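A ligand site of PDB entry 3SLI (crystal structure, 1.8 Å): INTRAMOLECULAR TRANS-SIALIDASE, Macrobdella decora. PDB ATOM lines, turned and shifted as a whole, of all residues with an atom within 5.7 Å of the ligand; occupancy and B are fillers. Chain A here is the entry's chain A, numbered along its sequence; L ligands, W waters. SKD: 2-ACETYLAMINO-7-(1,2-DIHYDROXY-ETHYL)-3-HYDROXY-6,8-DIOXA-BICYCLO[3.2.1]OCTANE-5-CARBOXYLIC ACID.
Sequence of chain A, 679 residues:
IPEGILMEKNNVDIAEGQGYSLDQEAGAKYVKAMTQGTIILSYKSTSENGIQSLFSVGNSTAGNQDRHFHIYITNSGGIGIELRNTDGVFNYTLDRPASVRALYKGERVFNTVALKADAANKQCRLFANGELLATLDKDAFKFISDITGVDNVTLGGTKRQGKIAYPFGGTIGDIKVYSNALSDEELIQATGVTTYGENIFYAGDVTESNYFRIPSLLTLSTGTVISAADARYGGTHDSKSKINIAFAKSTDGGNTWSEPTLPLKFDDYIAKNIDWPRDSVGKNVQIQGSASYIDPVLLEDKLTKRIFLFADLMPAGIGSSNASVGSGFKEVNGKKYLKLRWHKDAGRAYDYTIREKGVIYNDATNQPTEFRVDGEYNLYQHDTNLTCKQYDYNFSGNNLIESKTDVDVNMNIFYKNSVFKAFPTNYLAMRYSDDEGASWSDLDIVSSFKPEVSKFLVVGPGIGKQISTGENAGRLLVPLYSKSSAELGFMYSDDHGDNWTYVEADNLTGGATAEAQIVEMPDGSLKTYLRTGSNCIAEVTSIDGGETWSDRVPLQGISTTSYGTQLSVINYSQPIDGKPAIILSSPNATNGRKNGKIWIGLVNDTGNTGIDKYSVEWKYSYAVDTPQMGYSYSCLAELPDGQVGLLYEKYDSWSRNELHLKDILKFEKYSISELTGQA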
ATOM      1  N   ARG A 213      10.142  28.176 -32.761  1.00  0.00           N
ATOM      2  CA  ARG A 213       9.656  29.080 -31.716  1.00  0.00           C
ATOM      3  C   ARG A 213      10.861  29.625 -30.955  1.00  0.00           C
ATOM      4  O   ARG A 213      11.991  29.183 -31.172  1.00  0.00           O
ATOM      5  CB  ARG A 213       8.744  28.329 -30.720  1.00  0.00           C
ATOM      6  CG  ARG A 213       7.270  28.311 -31.084  1.00  0.00           C
ATOM      7  CD  ARG A 213       6.526  29.336 -30.254  1.00  0.00           C
ATOM      8  NE  ARG A 213       5.993  28.808 -29.011  1.00  0.00           N
ATOM      9  CZ  ARG A 213       5.895  29.460 -27.860  1.00  0.00           C
ATOM     10  NH1 ARG A 213       6.304  30.718 -27.711  1.00  0.00           N
ATOM     11  NH2 ARG A 213       5.333  28.846 -26.830  1.00  0.00           N
ATOM     12  N   ILE A 214      10.603  30.583 -30.067  1.00  0.00           N
ATOM     13  CA  ILE A 214      11.606  31.199 -29.197  1.00  0.00           C
ATOM     14  C   ILE A 214      12.814  31.793 -29.927  1.00  0.00           C
ATOM     15  O   ILE A 214      13.919  31.247 -29.873  1.00  0.00           O
ATOM     16  CB  ILE A 214      12.088  30.199 -28.111  1.00  0.00           C
ATOM     17  CG1 ILE A 214      10.970  29.220 -27.710  1.00  0.00           C
ATOM     18  CG2 ILE A 214      12.599  30.978 -26.900  1.00  0.00           C
ATOM     19  CD1 ILE A 214       9.660  29.868 -27.257  1.00  0.00           C
ATOM     20  N   ASP A 230      14.187  27.534 -31.237  1.00  0.00           N
ATOM     21  CA  ASP A 230      13.821  26.150 -30.955  1.00  0.00           C
ATOM     22  C   ASP A 230      13.378  25.576 -32.294  1.00  0.00           C
ATOM     23  O   ASP A 230      12.628  26.226 -33.027  1.00  0.00           O
ATOM     24  CB  ASP A 230      12.554  26.088 -30.066  1.00  0.00           C
ATOM     25  CG  ASP A 230      12.835  26.170 -28.579  1.00  0.00           C
ATOM     26  OD1 ASP A 230      13.889  26.680 -28.143  1.00  0.00           O
ATOM     27  OD2 ASP A 230      11.928  25.733 -27.826  1.00  0.00           O
ATOM     28  N   ARG A 232      11.179  22.990 -33.149  1.00  0.00           N
ATOM     29  CA  ARG A 232      10.178  22.136 -32.512  1.00  0.00           C
ATOM     30  C   ARG A 232       9.606  21.129 -33.515  1.00  0.00           C
ATOM     31  O   ARG A 232       8.769  21.462 -34.345  1.00  0.00           O
ATOM     32  CB  ARG A 232       9.082  22.996 -31.877  1.00  0.00           C
ATOM     33  CG  ARG A 232       9.630  23.942 -30.805  1.00  0.00           C
ATOM     34  CD  ARG A 232       8.556  24.564 -29.910  1.00  0.00           C
ATOM     35  NE  ARG A 232       9.185  25.307 -28.805  1.00  0.00           N
ATOM     36  CZ  ARG A 232       8.561  25.716 -27.703  1.00  0.00           C
ATOM     37  NH1 ARG A 232       7.270  25.482 -27.520  1.00  0.00           N
ATOM     38  NH2 ARG A 232       9.258  26.335 -26.749  1.00  0.00           N
ATOM     39  N   ASP A 238       5.749  22.754 -25.935  1.00  0.00           N
ATOM     40  CA  ASP A 238       6.945  23.010 -25.120  1.00  0.00           C
ATOM     41  C   ASP A 238       7.530  21.658 -24.751  1.00  0.00           C
ATOM     42  O   ASP A 238       6.889  20.627 -24.958  1.00  0.00           O
ATOM     43  CB  ASP A 238       6.620  23.697 -23.789  1.00  0.00           C
ATOM     44  CG  ASP A 238       5.809  24.955 -23.953  1.00  0.00           C
ATOM     45  OD1 ASP A 238       6.036  25.714 -24.919  1.00  0.00           O
ATOM     46  OD2 ASP A 238       4.946  25.191 -23.081  1.00  0.00           O
ATOM     47  N   SER A 239       8.671  21.679 -24.057  1.00  0.00           N
ATOM     48  CA  SER A 239       9.330  20.467 -23.648  1.00  0.00           C
ATOM     49  C   SER A 239       8.509  19.416 -22.950  1.00  0.00           C
ATOM     50  O   SER A 239       7.689  19.666 -22.057  1.00  0.00           O
ATOM     51  CB  SER A 239      10.643  20.730 -22.927  1.00  0.00           C
ATOM     52  OG  SER A 239      11.662  20.858 -23.912  1.00  0.00           O
ATOM     53  N   ILE A 294      15.521  23.509 -25.023  1.00  0.00           N
ATOM     54  CA  ILE A 294      14.461  24.493 -25.189  1.00  0.00           C
ATOM     55  C   ILE A 294      14.877  25.844 -24.622  1.00  0.00           C
ATOM     56  O   ILE A 294      15.650  25.897 -23.664  1.00  0.00           O
ATOM     57  CB  ILE A 294      13.138  23.984 -24.497  1.00  0.00           C
ATOM     58  CG1 ILE A 294      12.019  25.011 -24.609  1.00  0.00           C
ATOM     59  CG2 ILE A 294      13.404  23.634 -23.040  1.00  0.00           C
ATOM     60  CD1 ILE A 294      10.674  24.460 -24.198  1.00  0.00           C
ATOM     61  N   ASP A 295      14.418  26.903 -25.295  1.00  0.00           N
ATOM     62  CA  ASP A 295      14.668  28.304 -24.931  1.00  0.00           C
ATOM     63  C   ASP A 295      16.122  28.755 -25.031  1.00  0.00           C
ATOM     64  O   ASP A 295      16.871  28.698 -24.052  1.00  0.00           O
ATOM     65  CB  ASP A 295      14.121  28.597 -23.526  1.00  0.00           C
ATOM     66  CG  ASP A 295      12.599  28.578 -23.476  1.00  0.00           C
ATOM     67  OD1 ASP A 295      11.935  28.565 -24.535  1.00  0.00           O
ATOM     68  OD2 ASP A 295      12.049  28.580 -22.356  1.00  0.00           O
ATOM     69  N   ASP A 312      17.914  25.345 -22.064  1.00  0.00           N
ATOM     70  CA  ASP A 312      17.553  24.404 -21.016  1.00  0.00           C
ATOM     71  C   ASP A 312      17.727  23.001 -21.594  1.00  0.00           C
ATOM     72  O   ASP A 312      17.380  22.743 -22.747  1.00  0.00           O
ATOM     73  CB  ASP A 312      16.088  24.536 -20.595  1.00  0.00           C
ATOM     74  CG  ASP A 312      15.723  25.930 -20.105  1.00  0.00           C
ATOM     75  OD1 ASP A 312      16.577  26.645 -19.526  1.00  0.00           O
ATOM     76  OD2 ASP A 312      14.552  26.300 -20.308  1.00  0.00           O
ATOM     77  N   MET A 314      16.510  19.306 -21.147  1.00  0.00           N
ATOM     78  CA  MET A 314      15.436  18.498 -20.589  1.00  0.00           C
ATOM     79  C   MET A 314      15.665  17.006 -20.818  1.00  0.00           C
ATOM     80  O   MET A 314      15.726  16.563 -21.965  1.00  0.00           O
ATOM     81  CB  MET A 314      14.103  18.885 -21.226  1.00  0.00           C
ATOM     82  CG  MET A 314      13.695  20.306 -21.004  1.00  0.00           C
ATOM     83  SD  MET A 314      13.388  20.632 -19.273  1.00  0.00           S
ATOM     84  CE  MET A 314      12.882  22.324 -19.365  1.00  0.00           C
ATOM     85  N   SER A 320       9.453  21.688 -18.121  1.00  0.00           N
ATOM     86  CA  SER A 320       9.416  22.559 -16.946  1.00  0.00           C
ATOM     87  C   SER A 320       8.299  22.171 -15.962  1.00  0.00           C
ATOM     88  O   SER A 320       8.494  22.190 -14.744  1.00  0.00           O
ATOM     89  CB  SER A 320       9.209  24.001 -17.416  1.00  0.00           C
ATOM     90  OG  SER A 320       9.736  24.918 -16.483  1.00  0.00           O
ATOM     91  N   VAL A 458      15.463  27.794 -15.047  1.00  0.00           N
ATOM     92  CA  VAL A 458      15.618  27.909 -16.490  1.00  0.00           C
ATOM     93  C   VAL A 458      16.006  29.306 -16.966  1.00  0.00           C
ATOM     94  O   VAL A 458      15.947  30.264 -16.197  1.00  0.00           O
ATOM     95  CB  VAL A 458      14.292  27.456 -17.173  1.00  0.00           C
ATOM     96  CG1 VAL A 458      14.028  25.961 -16.911  1.00  0.00           C
ATOM     97  CG2 VAL A 458      13.112  28.278 -16.639  1.00  0.00           C
ATOM     98  N   TYR A 481      15.006  32.147 -14.282  1.00  0.00           N
ATOM     99  CA  TYR A 481      13.792  32.187 -13.475  1.00  0.00           C
ATOM    100  C   TYR A 481      13.537  30.789 -12.950  1.00  0.00           C
ATOM    101  O   TYR A 481      14.017  29.807 -13.529  1.00  0.00           O
ATOM    102  CB  TYR A 481      12.571  32.796 -14.174  1.00  0.00           C
ATOM    103  CG  TYR A 481      11.913  31.978 -15.250  1.00  0.00           C
ATOM    104  CD1 TYR A 481      12.322  32.084 -16.590  1.00  0.00           C
ATOM    105  CD2 TYR A 481      10.857  31.102 -14.941  1.00  0.00           C
ATOM    106  CE1 TYR A 481      11.691  31.340 -17.594  1.00  0.00           C
ATOM    107  CE2 TYR A 481      10.222  30.369 -15.940  1.00  0.00           C
ATOM    108  CZ  TYR A 481      10.643  30.494 -17.258  1.00  0.00           C
ATOM    109  OH  TYR A 481      10.030  29.748 -18.229  1.00  0.00           O
ATOM    110  N   THR A 513       6.331  32.430 -14.700  1.00  0.00           N
ATOM    111  CA  THR A 513       7.231  32.470 -15.846  1.00  0.00           C
ATOM    112  C   THR A 513       7.835  33.873 -15.943  1.00  0.00           C
ATOM    113  O   THR A 513       7.416  34.690 -16.750  1.00  0.00           O
ATOM    114  CB  THR A 513       6.468  32.087 -17.152  1.00  0.00           C
ATOM    115  OG1 THR A 513       5.797  30.830 -16.948  1.00  0.00           O
ATOM    116  CG2 THR A 513       7.415  31.947 -18.321  1.00  0.00           C
ATOM    117  N   GLU A 515      10.364  35.456 -17.311  1.00  0.00           N
ATOM    118  CA  GLU A 515      11.362  35.616 -18.359  1.00  0.00           C
ATOM    119  C   GLU A 515      11.786  37.084 -18.384  1.00  0.00           C
ATOM    120  O   GLU A 515      10.946  37.996 -18.412  1.00  0.00           O
ATOM    121  CB  GLU A 515      10.761  35.237 -19.705  1.00  0.00           C
ATOM    122  CG  GLU A 515      10.343  33.783 -19.785  1.00  0.00           C
ATOM    123  CD  GLU A 515       9.319  33.536 -20.873  1.00  0.00           C
ATOM    124  OE1 GLU A 515       8.469  34.427 -21.114  1.00  0.00           O
ATOM    125  OE2 GLU A 515       9.342  32.447 -21.474  1.00  0.00           O
ATOM    126  N   ARG A 531       8.728  39.570 -17.532  1.00  0.00           N
ATOM    127  CA  ARG A 531       7.359  39.100 -17.631  1.00  0.00           C
ATOM    128  C   ARG A 531       7.042  38.685 -16.189  1.00  0.00           C
ATOM    129  O   ARG A 531       7.939  38.253 -15.452  1.00  0.00           O
ATOM    130  CB  ARG A 531       7.310  37.882 -18.558  1.00  0.00           C
ATOM    131  CG  ARG A 531       6.010  37.088 -18.528  1.00  0.00           C
ATOM    132  CD  ARG A 531       6.160  35.826 -19.372  1.00  0.00           C
ATOM    133  NE  ARG A 531       4.979  34.958 -19.353  1.00  0.00           N
ATOM    134  CZ  ARG A 531       4.845  33.877 -20.135  1.00  0.00           C
ATOM    135  NH1 ARG A 531       5.805  33.549 -20.985  1.00  0.00           N
ATOM    136  NH2 ARG A 531       3.767  33.126 -20.043  1.00  0.00           N
ATOM    137  N   GLY A 564       1.081  36.707 -19.340  1.00  0.00           N
ATOM    138  CA  GLY A 564       2.264  37.333 -19.887  1.00  0.00           C
ATOM    139  C   GLY A 564       2.880  36.728 -21.135  1.00  0.00           C
ATOM    140  O   GLY A 564       2.458  35.668 -21.621  1.00  0.00           O
ATOM    141  N   ARG A 593      -2.150  37.046 -27.367  1.00  0.00           N
ATOM    142  CA  ARG A 593      -0.820  37.527 -27.748  1.00  0.00           C
ATOM    143  C   ARG A 593      -0.949  38.181 -29.114  1.00  0.00           C
ATOM    144  O   ARG A 593      -0.845  37.514 -30.149  1.00  0.00           O
ATOM    145  CB  ARG A 593       0.197  36.390 -27.774  1.00  0.00           C
ATOM    146  CG  ARG A 593       0.465  35.810 -26.389  1.00  0.00           C
ATOM    147  CD  ARG A 593       1.623  34.842 -26.381  1.00  0.00           C
ATOM    148  NE  ARG A 593       2.084  34.592 -25.013  1.00  0.00           N
ATOM    149  CZ  ARG A 593       2.781  33.528 -24.639  1.00  0.00           C
ATOM    150  NH1 ARG A 593       3.107  32.593 -25.524  1.00  0.00           N
ATOM    151  NH2 ARG A 593       3.193  33.411 -23.373  1.00  0.00           N
ATOM    152  N   TYR A 633       6.554  35.861 -28.849  1.00  0.00           N
ATOM    153  CA  TYR A 633       7.963  36.036 -28.496  1.00  0.00           C
ATOM    154  C   TYR A 633       8.712  36.795 -29.593  1.00  0.00           C
ATOM    155  O   TYR A 633       8.354  36.703 -30.785  1.00  0.00           O
ATOM    156  CB  TYR A 633       8.631  34.688 -28.223  1.00  0.00           C
ATOM    157  CG  TYR A 633       8.305  34.053 -26.883  1.00  0.00           C
ATOM    158  CD1 TYR A 633       7.011  34.141 -26.345  1.00  0.00           C
ATOM    159  CD2 TYR A 633       9.273  33.353 -26.170  1.00  0.00           C
ATOM    160  CE1 TYR A 633       6.701  33.550 -25.128  1.00  0.00           C
ATOM    161  CE2 TYR A 633       8.972  32.753 -24.946  1.00  0.00           C
ATOM    162  CZ  TYR A 633       7.693  32.858 -24.432  1.00  0.00           C
ATOM    163  OH  TYR A 633       7.405  32.286 -23.205  1.00  0.00           O
ATOM    164  N   SER A 653       1.172  32.404 -29.820  1.00  0.00           N
ATOM    165  CA  SER A 653       1.775  31.149 -29.367  1.00  0.00           C
ATOM    166  C   SER A 653       1.218  30.565 -28.063  1.00  0.00           C
ATOM    167  O   SER A 653       1.677  29.513 -27.622  1.00  0.00           O
ATOM    168  CB  SER A 653       3.292  31.283 -29.268  1.00  0.00           C
ATOM    169  OG  SER A 653       3.660  32.292 -28.338  1.00  0.00           O
ATOM    170  N   TRP A 654       0.276  31.257 -27.443  1.00  0.00           N
ATOM    171  CA  TRP A 654      -0.341  30.791 -26.203  1.00  0.00           C
ATOM    172  C   TRP A 654      -1.647  30.083 -26.545  1.00  0.00           C
ATOM    173  O   TRP A 654      -1.991  29.058 -25.933  1.00  0.00           O
ATOM    174  CB  TRP A 654      -0.628  31.990 -25.283  1.00  0.00           C
ATOM    175  CG  TRP A 654      -1.131  31.633 -23.895  1.00  0.00           C
ATOM    176  CD1 TRP A 654      -2.417  31.785 -23.415  1.00  0.00           C
ATOM    177  CD2 TRP A 654      -0.350  31.152 -22.794  1.00  0.00           C
ATOM    178  NE1 TRP A 654      -2.462  31.450 -22.082  1.00  0.00           N
ATOM    179  CE2 TRP A 654      -1.223  31.060 -21.674  1.00  0.00           C
ATOM    180  CE3 TRP A 654       0.993  30.806 -22.631  1.00  0.00           C
ATOM    181  CZ2 TRP A 654      -0.780  30.624 -20.413  1.00  0.00           C
ATOM    182  CZ3 TRP A 654       1.440  30.382 -21.375  1.00  0.00           C
ATOM    183  CH2 TRP A 654       0.550  30.292 -20.288  1.00  0.00           C
HETATM  184  C1  SKD L   1       5.229  30.501 -23.301  1.00  0.00           C
HETATM  185  C2  SKD L   1       6.185  29.389 -22.922  1.00  0.00           C
HETATM  186  C3  SKD L   1       7.173  29.055 -24.055  1.00  0.00           C
HETATM  187  C4  SKD L   1       8.510  28.603 -23.418  1.00  0.00           C
HETATM  188  C5  SKD L   1       8.270  27.765 -22.123  1.00  0.00           C
HETATM  189  C6  SKD L   1       7.274  28.501 -21.167  1.00  0.00           C
HETATM  190  C7  SKD L   1       5.968  27.710 -21.327  1.00  0.00           C
HETATM  191  C8  SKD L   1       4.951  27.958 -20.194  1.00  0.00           C
HETATM  192  C9  SKD L   1       5.436  27.407 -18.856  1.00  0.00           C
HETATM  193  C10 SKD L   1       9.708  26.358 -20.770  1.00  0.00           C
HETATM  194  C11 SKD L   1      11.070  26.134 -20.139  1.00  0.00           C
HETATM  195  N5  SKD L   1       9.533  27.484 -21.468  1.00  0.00           N
HETATM  196  O1A SKD L   1       4.942  30.667 -24.505  1.00  0.00           O
HETATM  197  O1B SKD L   1       4.716  31.188 -22.390  1.00  0.00           O
HETATM  198  O4  SKD L   1       9.277  27.844 -24.347  1.00  0.00           O
HETATM  199  O6  SKD L   1       6.950  29.752 -21.772  1.00  0.00           O
HETATM  200  O7  SKD L   1       5.422  28.223 -22.551  1.00  0.00           O
HETATM  201  O8  SKD L   1       4.714  29.357 -20.069  1.00  0.00           O
HETATM  202  O9  SKD L   1       6.309  28.339 -18.231  1.00  0.00           O
HETATM  203  O10 SKD L   1       8.798  25.539 -20.585  1.00  0.00           O
HETATM  204  O   HOH W   1       8.720  27.450 -17.497  1.00  0.00           O
HETATM  205  O   HOH W   2       3.647  27.117 -24.536  1.00  0.00           O
HETATM  206  O   HOH W   3       3.340  30.363 -17.918  1.00  0.00           O
HETATM  207  O   HOH W   4       9.268  22.861 -20.795  1.00  0.00           O
HETATM  208  O   HOH W   5       6.052  24.402 -20.331  1.00  0.00           O
HETATM  209  O   HOH W   6      10.866  30.449 -20.657  1.00  0.00           O
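OD1 of Asp 295 sits at hydrogen-bond distance from O4 of the ligand.
An oxygen (O6) of the ligand sits close to the side-chain hydroxyl (OH) of Tyr 633, at 2.9 Å.
NH2 of Arg 232 sits at hydrogen-bond distance from O4 of the ligand (2.8 Å).
The side-chain hydroxyl (OG1) of Thr 513 lies within hydrogen-bond range of an oxygen (O9) of the ligand (2.8 Å).
O1A of the ligand lies within salt-bridge range of NH1 of Arg 593, at 2.8 Å.
The guanidinium group of Arg 531 is in salt-bridge range of an oxygen (O1B) of the ligand, 3.0 Å away.
NH2 of Arg 213 is in salt-bridge range of O1A of the ligand (3.0 Å).
OD1 of Asp 230 is in hydrogen-bond range of N of Asp 295 (2.9 Å).
NH1 of Arg 531 is in hydrogen-bond range of OH of Tyr 633, 3.0 Å away.
The guanidinium group of Arg 232 is in salt-bridge range of the side-chain carboxylate of Asp 238 (2.9 Å).
The guanidinium group (NH1) of Arg 593 sits at hydrogen-bond distance from the side-chain hydroxyl (OG) of Ser 653 (2.9 Å).
NH2 of Arg 593 lies within hydrogen-bond range of O of Gly 564.
The guanidinium group of Arg 531 is in salt-bridge range of the side-chain carboxylate of Glu 515, at 2.8 Å.
The backbone NH (N) of Asp 230 is in hydrogen-bond range of the backbone carbonyl oxygen (O) of Arg 213 (2.7 Å).
O of Val 458 is in hydrogen-bond range of N of Tyr 481 (2.8 Å).
The side-chain carboxylate of Asp 238 lies close to an oxygen (O7) of the ligand (3.1 Å).
CD1 of Ile 214 touches O4 of the ligand (3.6 Å).
CD1 of Ile 294 touches O4 of the ligand, 3.7 Å away.
Asp 312 touches the ligand (OD2 to C11, 3.5 Å).
Ser 320 touches the ligand (CB to O10, 3.5 Å).
Tyr 481 touches the ligand.
Glu 515 touches the ligand (OE2 to O6, 3.6 Å).
CZ3 of Trp 654 touches O1B of the ligand, 3.5 Å away.
Hydrophobic or aromatic side chains that line the ligand: Ile 214, Ile 294, Tyr 633 and Trp 654.
Of the 21 residues printed, 15 come within 4 Å of the ligand.
The nearest printed residue that does not touch the ligand is Met 314 (4.3 Å).
Water W1 lies within hydrogen-bond range of an oxygen (O9) of the ligand (2.7 Å), the side-chain hydroxyl (OH) of Tyr 481 (2.7 Å) and the side-chain hydroxyl (OG) of Ser 320 (2.9 Å).
Water W4 lies within hydrogen-bond range of an oxygen (O10) of the ligand (2.7 Å) and the backbone NH (N) of Ser 320 (2.9 Å).
Water W3 lies within hydrogen-bond range of the side-chain hydroxyl (OG1) of Thr 513 and an oxygen (O8) of the ligand.
Water W2 lies within hydrogen-bond range of the side-chain carboxylate of Asp 238 (2.7 Å), an oxygen (O7) of the ligand (2.9 Å) and the guanidinium group of Arg 213 (3.3 Å).
Water W5 lies within hydrogen-bond range of O10 of the ligand and OD2 of Asp 238.
Water W6 lies within hydrogen-bond range of OE2 of Glu 515 (2.6 Å), OH of Tyr 481 (2.7 Å), OD2 of Asp 295 (2.8 Å) and N5 of the ligand (3.4 Å).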
